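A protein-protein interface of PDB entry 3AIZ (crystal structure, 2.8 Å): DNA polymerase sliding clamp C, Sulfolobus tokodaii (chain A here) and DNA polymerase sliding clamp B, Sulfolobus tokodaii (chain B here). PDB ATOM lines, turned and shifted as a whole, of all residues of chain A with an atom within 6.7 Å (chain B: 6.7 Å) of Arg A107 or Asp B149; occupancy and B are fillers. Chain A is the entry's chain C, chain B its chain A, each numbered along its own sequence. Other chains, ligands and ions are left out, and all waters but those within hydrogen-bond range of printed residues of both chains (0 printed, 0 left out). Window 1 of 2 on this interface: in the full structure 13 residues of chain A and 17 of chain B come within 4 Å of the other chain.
The guanidinium group of Arg B148 is in hydrogen-bond range of the side-chain hydroxyl of Tyr A105.
The side-chain hydroxyl of Tyr A105 is in hydrogen-bond range of the side-chain carboxylate of Asp B149 (2.6 Å).
The backbone NH (N) of Thr A108 lies within hydrogen-bond range of the backbone carbonyl oxygen (O) of Lys B178 (2.9 Å).
The backbone NH of Leu B180 sits at hydrogen-bond distance from the backbone carbonyl oxygen of Glu A106 (2.8 Å).
The guanidinium group (NH1) of Arg B148 lies within salt-bridge range of the side-chain carboxylate (OD1) of Asp B145 (3.9 Å).
The guanidinium group (NE) of Arg B148 lies within salt-bridge range of the side-chain carboxylate (OD1) of Asp B149 (3.1 Å).
The backbone carbonyl oxygen (O) of Arg B148 is in hydrogen-bond range of the side-chain hydroxyl (OG) of Ser B151 (2.6 Å).
The side-chain carboxylate (OD2) of Asp B149 sits at hydrogen-bond distance from the side-chain hydroxyl (OH) of Tyr B177 (2.9 Å).
OH of Tyr B177 lies close to OG of Ser B179 (3.1 Å).
The side-chain hydroxyl of Thr A108 lies within hydrogen-bond range of the side-chain hydroxyl of Thr A100, at 2.9 Å.
Among the printed residues, pairs that only touch across the chains: Arg A107 with Asp B149 (3.3 Å), Glu A106 with Ser B179 (3.3 Å), Phe A109 with Tyr B177 (3.3 Å), Thr A108 with Tyr B177 (3.5 Å), Tyr A105 with Asp B145 (3.5 Å), Thr A80 with Arg B148 (3.5 Å), Arg A107 with Lys B178 (3.6 Å), Phe A109 with Asp B149 (3.7 Å), Val A104 with Val B142 (3.8 Å), Tyr A105 with Ile B146 (3.8 Å), Phe A109 with Val B153 (3.9 Å), Arg A107 with Ser B179 (3.9 Å) and Tyr A105 with Tyr B177 (3.99 Å).
Asp A102 touches none of the printed residues of chain B.
Of the printed residues of chain B, Arg A107 touches Asp B149 (3.3 Å), Lys B178 (3.6 Å) and Ser B179 (3.9 Å).
Printed residues of chain B within 4 Å of Phe A109: Asp B149, Val B153 and Tyr B177.
Of the printed residues of chain A, Ile B146 touches Tyr A105.
Asp B149 touches just these residues of chain A: Tyr A105, Arg A107 and Phe A109.
Ser B151 touches none of the printed residues of chain A.
Printed residues of chain A within 4 Å of Val B153: Phe A109.
Of the printed residues of chain A, Lys B178 touches Arg A107 and Thr A108.
The nearest residue of chain A that does not touch Asp B149 is Thr A80 (4.4 Å).
The nearest printed residue of chain B that does not touch Phe A109 is Leu B152 (4.2 Å).
Printed residues of chain A that touch a printed residue of chain B: Thr A80, Val A104, Tyr A105, Glu A106, Arg A107, Thr A108 and Phe A109.
Hydrophobic or aromatic side chains of chain B within 4 Å of the printed part of chain A: Val B142, Ile B146, Val B153 and Tyr B177.
Among the printed residues, 17 pairs touch across the chains.
Among the printed residues, no Asp or Glu carboxylate lies within 4 Å of a Lys or Arg side-chain nitrogen of the other chain.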
ATOM      1  N   VAL A  77     -11.874  18.060 -20.639  1.00  0.00           N
ATOM      2  CA  VAL A  77     -10.983  17.751 -21.752  1.00  0.00           C
ATOM      3  C   VAL A  77     -10.296  19.009 -22.267  1.00  0.00           C
ATOM      4  O   VAL A  77      -9.226  18.937 -22.869  1.00  0.00           O
ATOM      5  CB  VAL A  77     -11.721  17.055 -22.917  1.00  0.00           C
ATOM      6  CG1 VAL A  77     -12.524  15.870 -22.403  1.00  0.00           C
ATOM      7  CG2 VAL A  77     -12.620  18.036 -23.642  1.00  0.00           C
ATOM      8  N   THR A  80      -6.982  19.880 -20.640  1.00  0.00           N
ATOM      9  CA  THR A  80      -5.856  19.043 -21.037  1.00  0.00           C
ATOM     10  C   THR A  80      -5.139  19.579 -22.271  1.00  0.00           C
ATOM     11  O   THR A  80      -4.308  18.887 -22.859  1.00  0.00           O
ATOM     12  CB  THR A  80      -6.297  17.592 -21.310  1.00  0.00           C
ATOM     13  OG1 THR A  80      -6.961  17.519 -22.577  1.00  0.00           O
ATOM     14  CG2 THR A  80      -7.233  17.104 -20.215  1.00  0.00           C
ATOM     15  N   VAL A  81      -5.463  20.806 -22.666  1.00  0.00           N
ATOM     16  CA  VAL A  81      -4.817  21.416 -23.824  1.00  0.00           C
ATOM     17  C   VAL A  81      -3.507  22.084 -23.425  1.00  0.00           C
ATOM     18  O   VAL A  81      -3.382  22.625 -22.326  1.00  0.00           O
ATOM     19  CB  VAL A  81      -5.725  22.451 -24.520  1.00  0.00           C
ATOM     20  CG1 VAL A  81      -7.058  21.821 -24.893  1.00  0.00           C
ATOM     21  CG2 VAL A  81      -5.931  23.665 -23.631  1.00  0.00           C
ATOM     22  N   THR A  82      -2.531  22.039 -24.324  1.00  0.00           N
ATOM     23  CA  THR A  82      -1.237  22.660 -24.081  1.00  0.00           C
ATOM     24  C   THR A  82      -1.136  23.987 -24.822  1.00  0.00           C
ATOM     25  O   THR A  82      -2.121  24.477 -25.376  1.00  0.00           O
ATOM     26  CB  THR A  82      -0.084  21.747 -24.526  1.00  0.00           C
ATOM     27  OG1 THR A  82      -0.144  21.555 -25.945  1.00  0.00           O
ATOM     28  CG2 THR A  82      -0.176  20.398 -23.832  1.00  0.00           C
ATOM     29  N   ASP A  85      -1.296  23.236 -28.751  1.00  0.00           N
ATOM     30  CA  ASP A  85      -2.406  22.383 -29.161  1.00  0.00           C
ATOM     31  C   ASP A  85      -3.402  23.148 -30.019  1.00  0.00           C
ATOM     32  O   ASP A  85      -3.798  24.261 -29.679  1.00  0.00           O
ATOM     33  CB  ASP A  85      -3.129  21.814 -27.940  1.00  0.00           C
ATOM     34  CG  ASP A  85      -2.587  20.469 -27.515  1.00  0.00           C
ATOM     35  OD1 ASP A  85      -2.041  19.748 -28.378  1.00  0.00           O
ATOM     36  OD2 ASP A  85      -2.713  20.128 -26.321  1.00  0.00           O
ATOM     37  N   VAL A  99     -14.585  16.710 -29.914  1.00  0.00           N
ATOM     38  CA  VAL A  99     -13.462  17.580 -29.596  1.00  0.00           C
ATOM     39  C   VAL A  99     -12.160  16.872 -29.947  1.00  0.00           C
ATOM     40  O   VAL A  99     -11.844  15.822 -29.387  1.00  0.00           O
ATOM     41  CB  VAL A  99     -13.447  17.962 -28.106  1.00  0.00           C
ATOM     42  CG1 VAL A  99     -12.421  19.053 -27.849  1.00  0.00           C
ATOM     43  CG2 VAL A  99     -14.825  18.417 -27.663  1.00  0.00           C
ATOM     44  N   THR A 100     -11.408  17.445 -30.880  1.00  0.00           N
ATOM     45  CA  THR A 100     -10.161  16.838 -31.327  1.00  0.00           C
ATOM     46  C   THR A 100      -8.958  17.712 -30.999  1.00  0.00           C
ATOM     47  O   THR A 100      -8.729  18.733 -31.646  1.00  0.00           O
ATOM     48  CB  THR A 100     -10.178  16.564 -32.840  1.00  0.00           C
ATOM     49  OG1 THR A 100     -11.285  15.713 -33.160  1.00  0.00           O
ATOM     50  CG2 THR A 100      -8.884  15.894 -33.275  1.00  0.00           C
ATOM     51  N   LEU A 101      -8.192  17.305 -29.994  1.00  0.00           N
ATOM     52  CA  LEU A 101      -6.971  18.012 -29.634  1.00  0.00           C
ATOM     53  C   LEU A 101      -5.806  17.495 -30.472  1.00  0.00           C
ATOM     54  O   LEU A 101      -5.551  16.292 -30.524  1.00  0.00           O
ATOM     55  CB  LEU A 101      -6.671  17.841 -28.145  1.00  0.00           C
ATOM     56  CG  LEU A 101      -7.803  18.232 -27.197  1.00  0.00           C
ATOM     57  CD1 LEU A 101      -7.337  18.166 -25.754  1.00  0.00           C
ATOM     58  CD2 LEU A 101      -8.317  19.622 -27.527  1.00  0.00           C
ATOM     59  N   ASP A 102      -5.104  18.410 -31.133  1.00  0.00           N
ATOM     60  CA  ASP A 102      -4.009  18.035 -32.015  1.00  0.00           C
ATOM     61  C   ASP A 102      -2.715  18.737 -31.619  1.00  0.00           C
ATOM     62  O   ASP A 102      -2.588  19.953 -31.761  1.00  0.00           O
ATOM     63  CB  ASP A 102      -4.365  18.360 -33.468  1.00  0.00           C
ATOM     64  CG  ASP A 102      -3.392  17.749 -34.460  1.00  0.00           C
ATOM     65  OD1 ASP A 102      -2.301  17.310 -34.037  1.00  0.00           O
ATOM     66  OD2 ASP A 102      -3.720  17.709 -35.665  1.00  0.00           O
ATOM     67  N   GLY A 103      -1.759  17.959 -31.121  1.00  0.00           N
ATOM     68  CA  GLY A 103      -0.466  18.485 -30.726  1.00  0.00           C
ATOM     69  C   GLY A 103       0.602  17.412 -30.790  1.00  0.00           C
ATOM     70  O   GLY A 103       0.852  16.839 -31.850  1.00  0.00           O
ATOM     71  N   VAL A 104       1.235  17.140 -29.651  1.00  0.00           N
ATOM     72  CA  VAL A 104       2.222  16.071 -29.565  1.00  0.00           C
ATOM     73  C   VAL A 104       1.638  14.780 -30.128  1.00  0.00           C
ATOM     74  O   VAL A 104       2.317  14.026 -30.825  1.00  0.00           O
ATOM     75  CB  VAL A 104       2.667  15.835 -28.112  1.00  0.00           C
ATOM     76  CG1 VAL A 104       3.620  14.648 -28.035  1.00  0.00           C
ATOM     77  CG2 VAL A 104       3.314  17.091 -27.545  1.00  0.00           C
ATOM     78  N   TYR A 105       0.371  14.535 -29.817  1.00  0.00           N
ATOM     79  CA  TYR A 105      -0.360  13.404 -30.373  1.00  0.00           C
ATOM     80  C   TYR A 105      -1.803  13.819 -30.616  1.00  0.00           C
ATOM     81  O   TYR A 105      -2.287  14.774 -30.010  1.00  0.00           O
ATOM     82  CB  TYR A 105      -0.299  12.202 -29.430  1.00  0.00           C
ATOM     83  CG  TYR A 105      -1.007  12.416 -28.112  1.00  0.00           C
ATOM     84  CD1 TYR A 105      -0.488  13.276 -27.154  1.00  0.00           C
ATOM     85  CD2 TYR A 105      -2.190  11.751 -27.822  1.00  0.00           C
ATOM     86  CE1 TYR A 105      -1.130  13.471 -25.949  1.00  0.00           C
ATOM     87  CE2 TYR A 105      -2.837  11.940 -26.618  1.00  0.00           C
ATOM     88  CZ  TYR A 105      -2.303  12.801 -25.685  1.00  0.00           C
ATOM     89  OH  TYR A 105      -2.943  12.994 -24.484  1.00  0.00           O
ATOM     90  N   GLU A 106      -2.488  13.111 -31.506  1.00  0.00           N
ATOM     91  CA  GLU A 106      -3.870  13.443 -31.831  1.00  0.00           C
ATOM     92  C   GLU A 106      -4.842  12.619 -30.992  1.00  0.00           C
ATOM     93  O   GLU A 106      -4.651  11.418 -30.804  1.00  0.00           O
ATOM     94  CB  GLU A 106      -4.138  13.237 -33.322  1.00  0.00           C
ATOM     95  CG  GLU A 106      -5.448  13.838 -33.800  1.00  0.00           C
ATOM     96  CD  GLU A 106      -5.640  13.691 -35.296  1.00  0.00           C
ATOM     97  OE1 GLU A 106      -5.066  12.745 -35.878  1.00  0.00           O
ATOM     98  OE2 GLU A 106      -6.366  14.520 -35.888  1.00  0.00           O
ATOM     99  N   ARG A 107      -5.883  13.272 -30.491  1.00  0.00           N
ATOM    100  CA  ARG A 107      -6.848  12.621 -29.613  1.00  0.00           C
ATOM    101  C   ARG A 107      -8.237  13.226 -29.790  1.00  0.00           C
ATOM    102  O   ARG A 107      -8.379  14.436 -29.957  1.00  0.00           O
ATOM    103  CB  ARG A 107      -6.395  12.745 -28.158  1.00  0.00           C
ATOM    104  CG  ARG A 107      -6.062  14.171 -27.741  1.00  0.00           C
ATOM    105  CD  ARG A 107      -5.306  14.206 -26.425  1.00  0.00           C
ATOM    106  NE  ARG A 107      -4.954  15.566 -26.023  1.00  0.00           N
ATOM    107  CZ  ARG A 107      -3.986  16.285 -26.585  1.00  0.00           C
ATOM    108  NH1 ARG A 107      -3.732  17.512 -26.154  1.00  0.00           N
ATOM    109  NH2 ARG A 107      -3.277  15.780 -27.583  1.00  0.00           N
ATOM    110  N   THR A 108      -9.261  12.378 -29.752  1.00  0.00           N
ATOM    111  CA  THR A 108     -10.632  12.835 -29.950  1.00  0.00           C
ATOM    112  C   THR A 108     -11.581  12.362 -28.853  1.00  0.00           C
ATOM    113  O   THR A 108     -11.784  11.162 -28.664  1.00  0.00           O
ATOM    114  CB  THR A 108     -11.186  12.388 -31.315  1.00  0.00           C
ATOM    115  OG1 THR A 108     -10.490  13.073 -32.364  1.00  0.00           O
ATOM    116  CG2 THR A 108     -12.673  12.701 -31.414  1.00  0.00           C
ATOM    117  N   PHE A 109     -12.158  13.319 -28.133  1.00  0.00           N
ATOM    118  CA  PHE A 109     -13.181  13.027 -27.138  1.00  0.00           C
ATOM    119  C   PHE A 109     -14.564  13.261 -27.738  1.00  0.00           C
ATOM    120  O   PHE A 109     -14.740  14.124 -28.598  1.00  0.00           O
ATOM    121  CB  PHE A 109     -13.002  13.913 -25.904  1.00  0.00           C
ATOM    122  CG  PHE A 109     -11.733  13.657 -25.145  1.00  0.00           C
ATOM    123  CD1 PHE A 109     -10.542  14.237 -25.543  1.00  0.00           C
ATOM    124  CD2 PHE A 109     -11.736  12.850 -24.019  1.00  0.00           C
ATOM    125  CE1 PHE A 109      -9.376  14.008 -24.842  1.00  0.00           C
ATOM    126  CE2 PHE A 109     -10.573  12.619 -23.313  1.00  0.00           C
ATOM    127  CZ  PHE A 109      -9.392  13.198 -23.725  1.00  0.00           C
ATOM    128  N   VAL B 142       4.199  11.435 -22.806  1.00  0.00           N
ATOM    129  CA  VAL B 142       3.062  11.199 -23.684  1.00  0.00           C
ATOM    130  C   VAL B 142       2.123  10.161 -23.083  1.00  0.00           C
ATOM    131  O   VAL B 142       0.914  10.377 -23.004  1.00  0.00           O
ATOM    132  CB  VAL B 142       3.509  10.727 -25.078  1.00  0.00           C
ATOM    133  CG1 VAL B 142       2.297  10.448 -25.951  1.00  0.00           C
ATOM    134  CG2 VAL B 142       4.414  11.764 -25.725  1.00  0.00           C
ATOM    135  N   LYS B 144       1.864   9.337 -20.044  1.00  0.00           N
ATOM    136  CA  LYS B 144       1.264   9.956 -18.871  1.00  0.00           C
ATOM    137  C   LYS B 144       0.063  10.801 -19.281  1.00  0.00           C
ATOM    138  O   LYS B 144      -0.982  10.761 -18.634  1.00  0.00           O
ATOM    139  CB  LYS B 144       2.290  10.816 -18.134  1.00  0.00           C
ATOM    140  CG  LYS B 144       1.789  11.401 -16.823  1.00  0.00           C
ATOM    141  CD  LYS B 144       2.907  12.127 -16.095  1.00  0.00           C
ATOM    142  CE  LYS B 144       2.468  12.586 -14.716  1.00  0.00           C
ATOM    143  NZ  LYS B 144       3.588  13.229 -13.970  1.00  0.00           N
ATOM    144  N   ASP B 145       0.217  11.560 -20.361  1.00  0.00           N
ATOM    145  CA  ASP B 145      -0.879  12.361 -20.896  1.00  0.00           C
ATOM    146  C   ASP B 145      -2.059  11.477 -21.286  1.00  0.00           C
ATOM    147  O   ASP B 145      -3.211  11.800 -20.996  1.00  0.00           O
ATOM    148  CB  ASP B 145      -0.413  13.183 -22.100  1.00  0.00           C
ATOM    149  CG  ASP B 145       0.510  14.322 -21.708  1.00  0.00           C
ATOM    150  OD1 ASP B 145       0.461  14.751 -20.535  1.00  0.00           O
ATOM    151  OD2 ASP B 145       1.281  14.793 -22.573  1.00  0.00           O
ATOM    152  N   ILE B 146      -1.766  10.360 -21.943  1.00  0.00           N
ATOM    153  CA  ILE B 146      -2.795   9.403 -22.333  1.00  0.00           C
ATOM    154  C   ILE B 146      -3.477   8.802 -21.106  1.00  0.00           C
ATOM    155  O   ILE B 146      -4.673   8.513 -21.127  1.00  0.00           O
ATOM    156  CB  ILE B 146      -2.214   8.275 -23.204  1.00  0.00           C
ATOM    157  CG1 ILE B 146      -1.716   8.838 -24.536  1.00  0.00           C
ATOM    158  CG2 ILE B 146      -3.251   7.191 -23.441  1.00  0.00           C
ATOM    159  CD1 ILE B 146      -1.155   7.792 -25.469  1.00  0.00           C
ATOM    160  N   ALA B 147      -2.711   8.619 -20.035  1.00  0.00           N
ATOM    161  CA  ALA B 147      -3.261   8.106 -18.788  1.00  0.00           C
ATOM    162  C   ALA B 147      -4.278   9.088 -18.215  1.00  0.00           C
ATOM    163  O   ALA B 147      -5.332   8.690 -17.721  1.00  0.00           O
ATOM    164  CB  ALA B 147      -2.152   7.838 -17.787  1.00  0.00           C
ATOM    165  N   ARG B 148      -3.951  10.374 -18.284  1.00  0.00           N
ATOM    166  CA  ARG B 148      -4.861  11.423 -17.843  1.00  0.00           C
ATOM    167  C   ARG B 148      -6.141  11.406 -18.674  1.00  0.00           C
ATOM    168  O   ARG B 148      -7.244  11.527 -18.138  1.00  0.00           O
ATOM    169  CB  ARG B 148      -4.187  12.789 -17.949  1.00  0.00           C
ATOM    170  CG  ARG B 148      -5.150  13.961 -17.901  1.00  0.00           C
ATOM    171  CD  ARG B 148      -4.595  15.134 -18.684  1.00  0.00           C
ATOM    172  NE  ARG B 148      -4.280  14.755 -20.058  1.00  0.00           N
ATOM    173  CZ  ARG B 148      -3.530  15.479 -20.881  1.00  0.00           C
ATOM    174  NH1 ARG B 148      -3.010  16.628 -20.469  1.00  0.00           N
ATOM    175  NH2 ARG B 148      -3.294  15.053 -22.114  1.00  0.00           N
ATOM    176  N   ASP B 149      -5.988  11.259 -19.985  1.00  0.00           N
ATOM    177  CA  ASP B 149      -7.133  11.165 -20.880  1.00  0.00           C
ATOM    178  C   ASP B 149      -8.025   9.999 -20.479  1.00  0.00           C
ATOM    179  O   ASP B 149      -9.233  10.158 -20.311  1.00  0.00           O
ATOM    180  CB  ASP B 149      -6.671  10.987 -22.326  1.00  0.00           C
ATOM    181  CG  ASP B 149      -5.905  12.184 -22.846  1.00  0.00           C
ATOM    182  OD1 ASP B 149      -5.897  13.231 -22.165  1.00  0.00           O
ATOM    183  OD2 ASP B 149      -5.313  12.079 -23.941  1.00  0.00           O
ATOM    184  N   LEU B 150      -7.418   8.827 -20.323  1.00  0.00           N
ATOM    185  CA  LEU B 150      -8.156   7.617 -19.979  1.00  0.00           C
ATOM    186  C   LEU B 150      -8.860   7.736 -18.630  1.00  0.00           C
ATOM    187  O   LEU B 150      -9.935   7.172 -18.432  1.00  0.00           O
ATOM    188  CB  LEU B 150      -7.224   6.402 -19.985  1.00  0.00           C
ATOM    189  CG  LEU B 150      -6.611   6.056 -21.345  1.00  0.00           C
ATOM    190  CD1 LEU B 150      -5.526   4.999 -21.203  1.00  0.00           C
ATOM    191  CD2 LEU B 150      -7.685   5.608 -22.325  1.00  0.00           C
ATOM    192  N   SER B 151      -8.255   8.477 -17.706  1.00  0.00           N
ATOM    193  CA  SER B 151      -8.838   8.656 -16.381  1.00  0.00           C
ATOM    194  C   SER B 151     -10.075   9.548 -16.445  1.00  0.00           C
ATOM    195  O   SER B 151     -10.672   9.874 -15.418  1.00  0.00           O
ATOM    196  CB  SER B 151      -7.816   9.249 -15.410  1.00  0.00           C
ATOM    197  OG  SER B 151      -7.598  10.623 -15.676  1.00  0.00           O
ATOM    198  N   LEU B 152     -10.454   9.940 -17.656  1.00  0.00           N
ATOM    199  CA  LEU B 152     -11.631  10.774 -17.852  1.00  0.00           C
ATOM    200  C   LEU B 152     -12.832   9.972 -18.339  1.00  0.00           C
ATOM    201  O   LEU B 152     -13.947  10.162 -17.856  1.00  0.00           O
ATOM    202  CB  LEU B 152     -11.338  11.908 -18.836  1.00  0.00           C
ATOM    203  CG  LEU B 152     -10.491  13.074 -18.322  1.00  0.00           C
ATOM    204  CD1 LEU B 152     -10.236  14.076 -19.436  1.00  0.00           C
ATOM    205  CD2 LEU B 152     -11.172  13.742 -17.142  1.00  0.00           C
ATOM    206  N   VAL B 153     -12.603   9.072 -19.287  1.00  0.00           N
ATOM    207  CA  VAL B 153     -13.710   8.411 -19.971  1.00  0.00           C
ATOM    208  C   VAL B 153     -13.928   6.944 -19.590  1.00  0.00           C
ATOM    209  O   VAL B 153     -14.579   6.643 -18.591  1.00  0.00           O
ATOM    210  CB  VAL B 153     -13.560   8.515 -21.503  1.00  0.00           C
ATOM    211  CG1 VAL B 153     -14.888   8.227 -22.180  1.00  0.00           C
ATOM    212  CG2 VAL B 153     -13.055   9.892 -21.890  1.00  0.00           C
ATOM    213  N   GLY B 154     -13.376   6.039 -20.392  1.00  0.00           N
ATOM    214  CA  GLY B 154     -13.755   4.636 -20.349  1.00  0.00           C
ATOM    215  C   GLY B 154     -13.420   3.844 -19.101  1.00  0.00           C
ATOM    216  O   GLY B 154     -13.063   4.401 -18.063  1.00  0.00           O
ATOM    217  N   THR B 170     -11.677   4.081 -25.770  1.00  0.00           N
ATOM    218  CA  THR B 170     -12.508   3.766 -24.614  1.00  0.00           C
ATOM    219  C   THR B 170     -13.904   4.354 -24.779  1.00  0.00           C
ATOM    220  O   THR B 170     -14.106   5.283 -25.562  1.00  0.00           O
ATOM    221  CB  THR B 170     -11.897   4.296 -23.304  1.00  0.00           C
ATOM    222  OG1 THR B 170     -11.761   5.721 -23.378  1.00  0.00           O
ATOM    223  CG2 THR B 170     -10.537   3.675 -23.064  1.00  0.00           C
ATOM    224  N   TYR B 177     -13.483   8.157 -26.207  1.00  0.00           N
ATOM    225  CA  TYR B 177     -12.111   8.631 -26.340  1.00  0.00           C
ATOM    226  C   TYR B 177     -11.353   7.791 -27.359  1.00  0.00           C
ATOM    227  O   TYR B 177     -11.495   6.570 -27.396  1.00  0.00           O
ATOM    228  CB  TYR B 177     -11.388   8.593 -24.993  1.00  0.00           C
ATOM    229  CG  TYR B 177      -9.902   8.861 -25.093  1.00  0.00           C
ATOM    230  CD1 TYR B 177      -9.417  10.156 -25.207  1.00  0.00           C
ATOM    231  CD2 TYR B 177      -8.985   7.820 -25.073  1.00  0.00           C
ATOM    232  CE1 TYR B 177      -8.062  10.407 -25.297  1.00  0.00           C
ATOM    233  CE2 TYR B 177      -7.628   8.061 -25.163  1.00  0.00           C
ATOM    234  CZ  TYR B 177      -7.172   9.356 -25.273  1.00  0.00           C
ATOM    235  OH  TYR B 177      -5.820   9.601 -25.362  1.00  0.00           O
ATOM    236  N   LYS B 178     -10.547   8.452 -28.182  1.00  0.00           N
ATOM    237  CA  LYS B 178      -9.749   7.760 -29.186  1.00  0.00           C
ATOM    238  C   LYS B 178      -8.525   8.574 -29.590  1.00  0.00           C
ATOM    239  O   LYS B 178      -8.641   9.583 -30.285  1.00  0.00           O
ATOM    240  CB  LYS B 178     -10.597   7.441 -30.419  1.00  0.00           C
ATOM    241  CG  LYS B 178      -9.850   6.671 -31.498  1.00  0.00           C
ATOM    242  CD  LYS B 178     -10.733   6.419 -32.710  1.00  0.00           C
ATOM    243  CE  LYS B 178     -11.981   5.633 -32.333  1.00  0.00           C
ATOM    244  NZ  LYS B 178     -12.890   5.440 -33.499  1.00  0.00           N
ATOM    245  N   SER B 179      -7.351   8.130 -29.149  1.00  0.00           N
ATOM    246  CA  SER B 179      -6.099   8.782 -29.516  1.00  0.00           C
ATOM    247  C   SER B 179      -5.353   7.975 -30.571  1.00  0.00           C
ATOM    248  O   SER B 179      -5.511   6.757 -30.662  1.00  0.00           O
ATOM    249  CB  SER B 179      -5.213   8.987 -28.286  1.00  0.00           C
ATOM    250  OG  SER B 179      -4.940   7.757 -27.639  1.00  0.00           O
ATOM    251  N   LEU B 180      -4.544   8.662 -31.369  1.00  0.00           N
ATOM    252  CA  LEU B 180      -3.786   8.015 -32.433  1.00  0.00           C
ATOM    253  C   LEU B 180      -2.301   8.325 -32.307  1.00  0.00           C
ATOM    254  O   LEU B 180      -1.900   9.488 -32.264  1.00  0.00           O
ATOM    255  CB  LEU B 180      -4.293   8.468 -33.803  1.00  0.00           C
ATOM    256  CG  LEU B 180      -5.790   8.296 -34.062  1.00  0.00           C
ATOM    257  CD1 LEU B 180      -6.174   8.887 -35.410  1.00  0.00           C
ATOM    258  CD2 LEU B 180      -6.186   6.830 -33.981  1.00  0.00           C
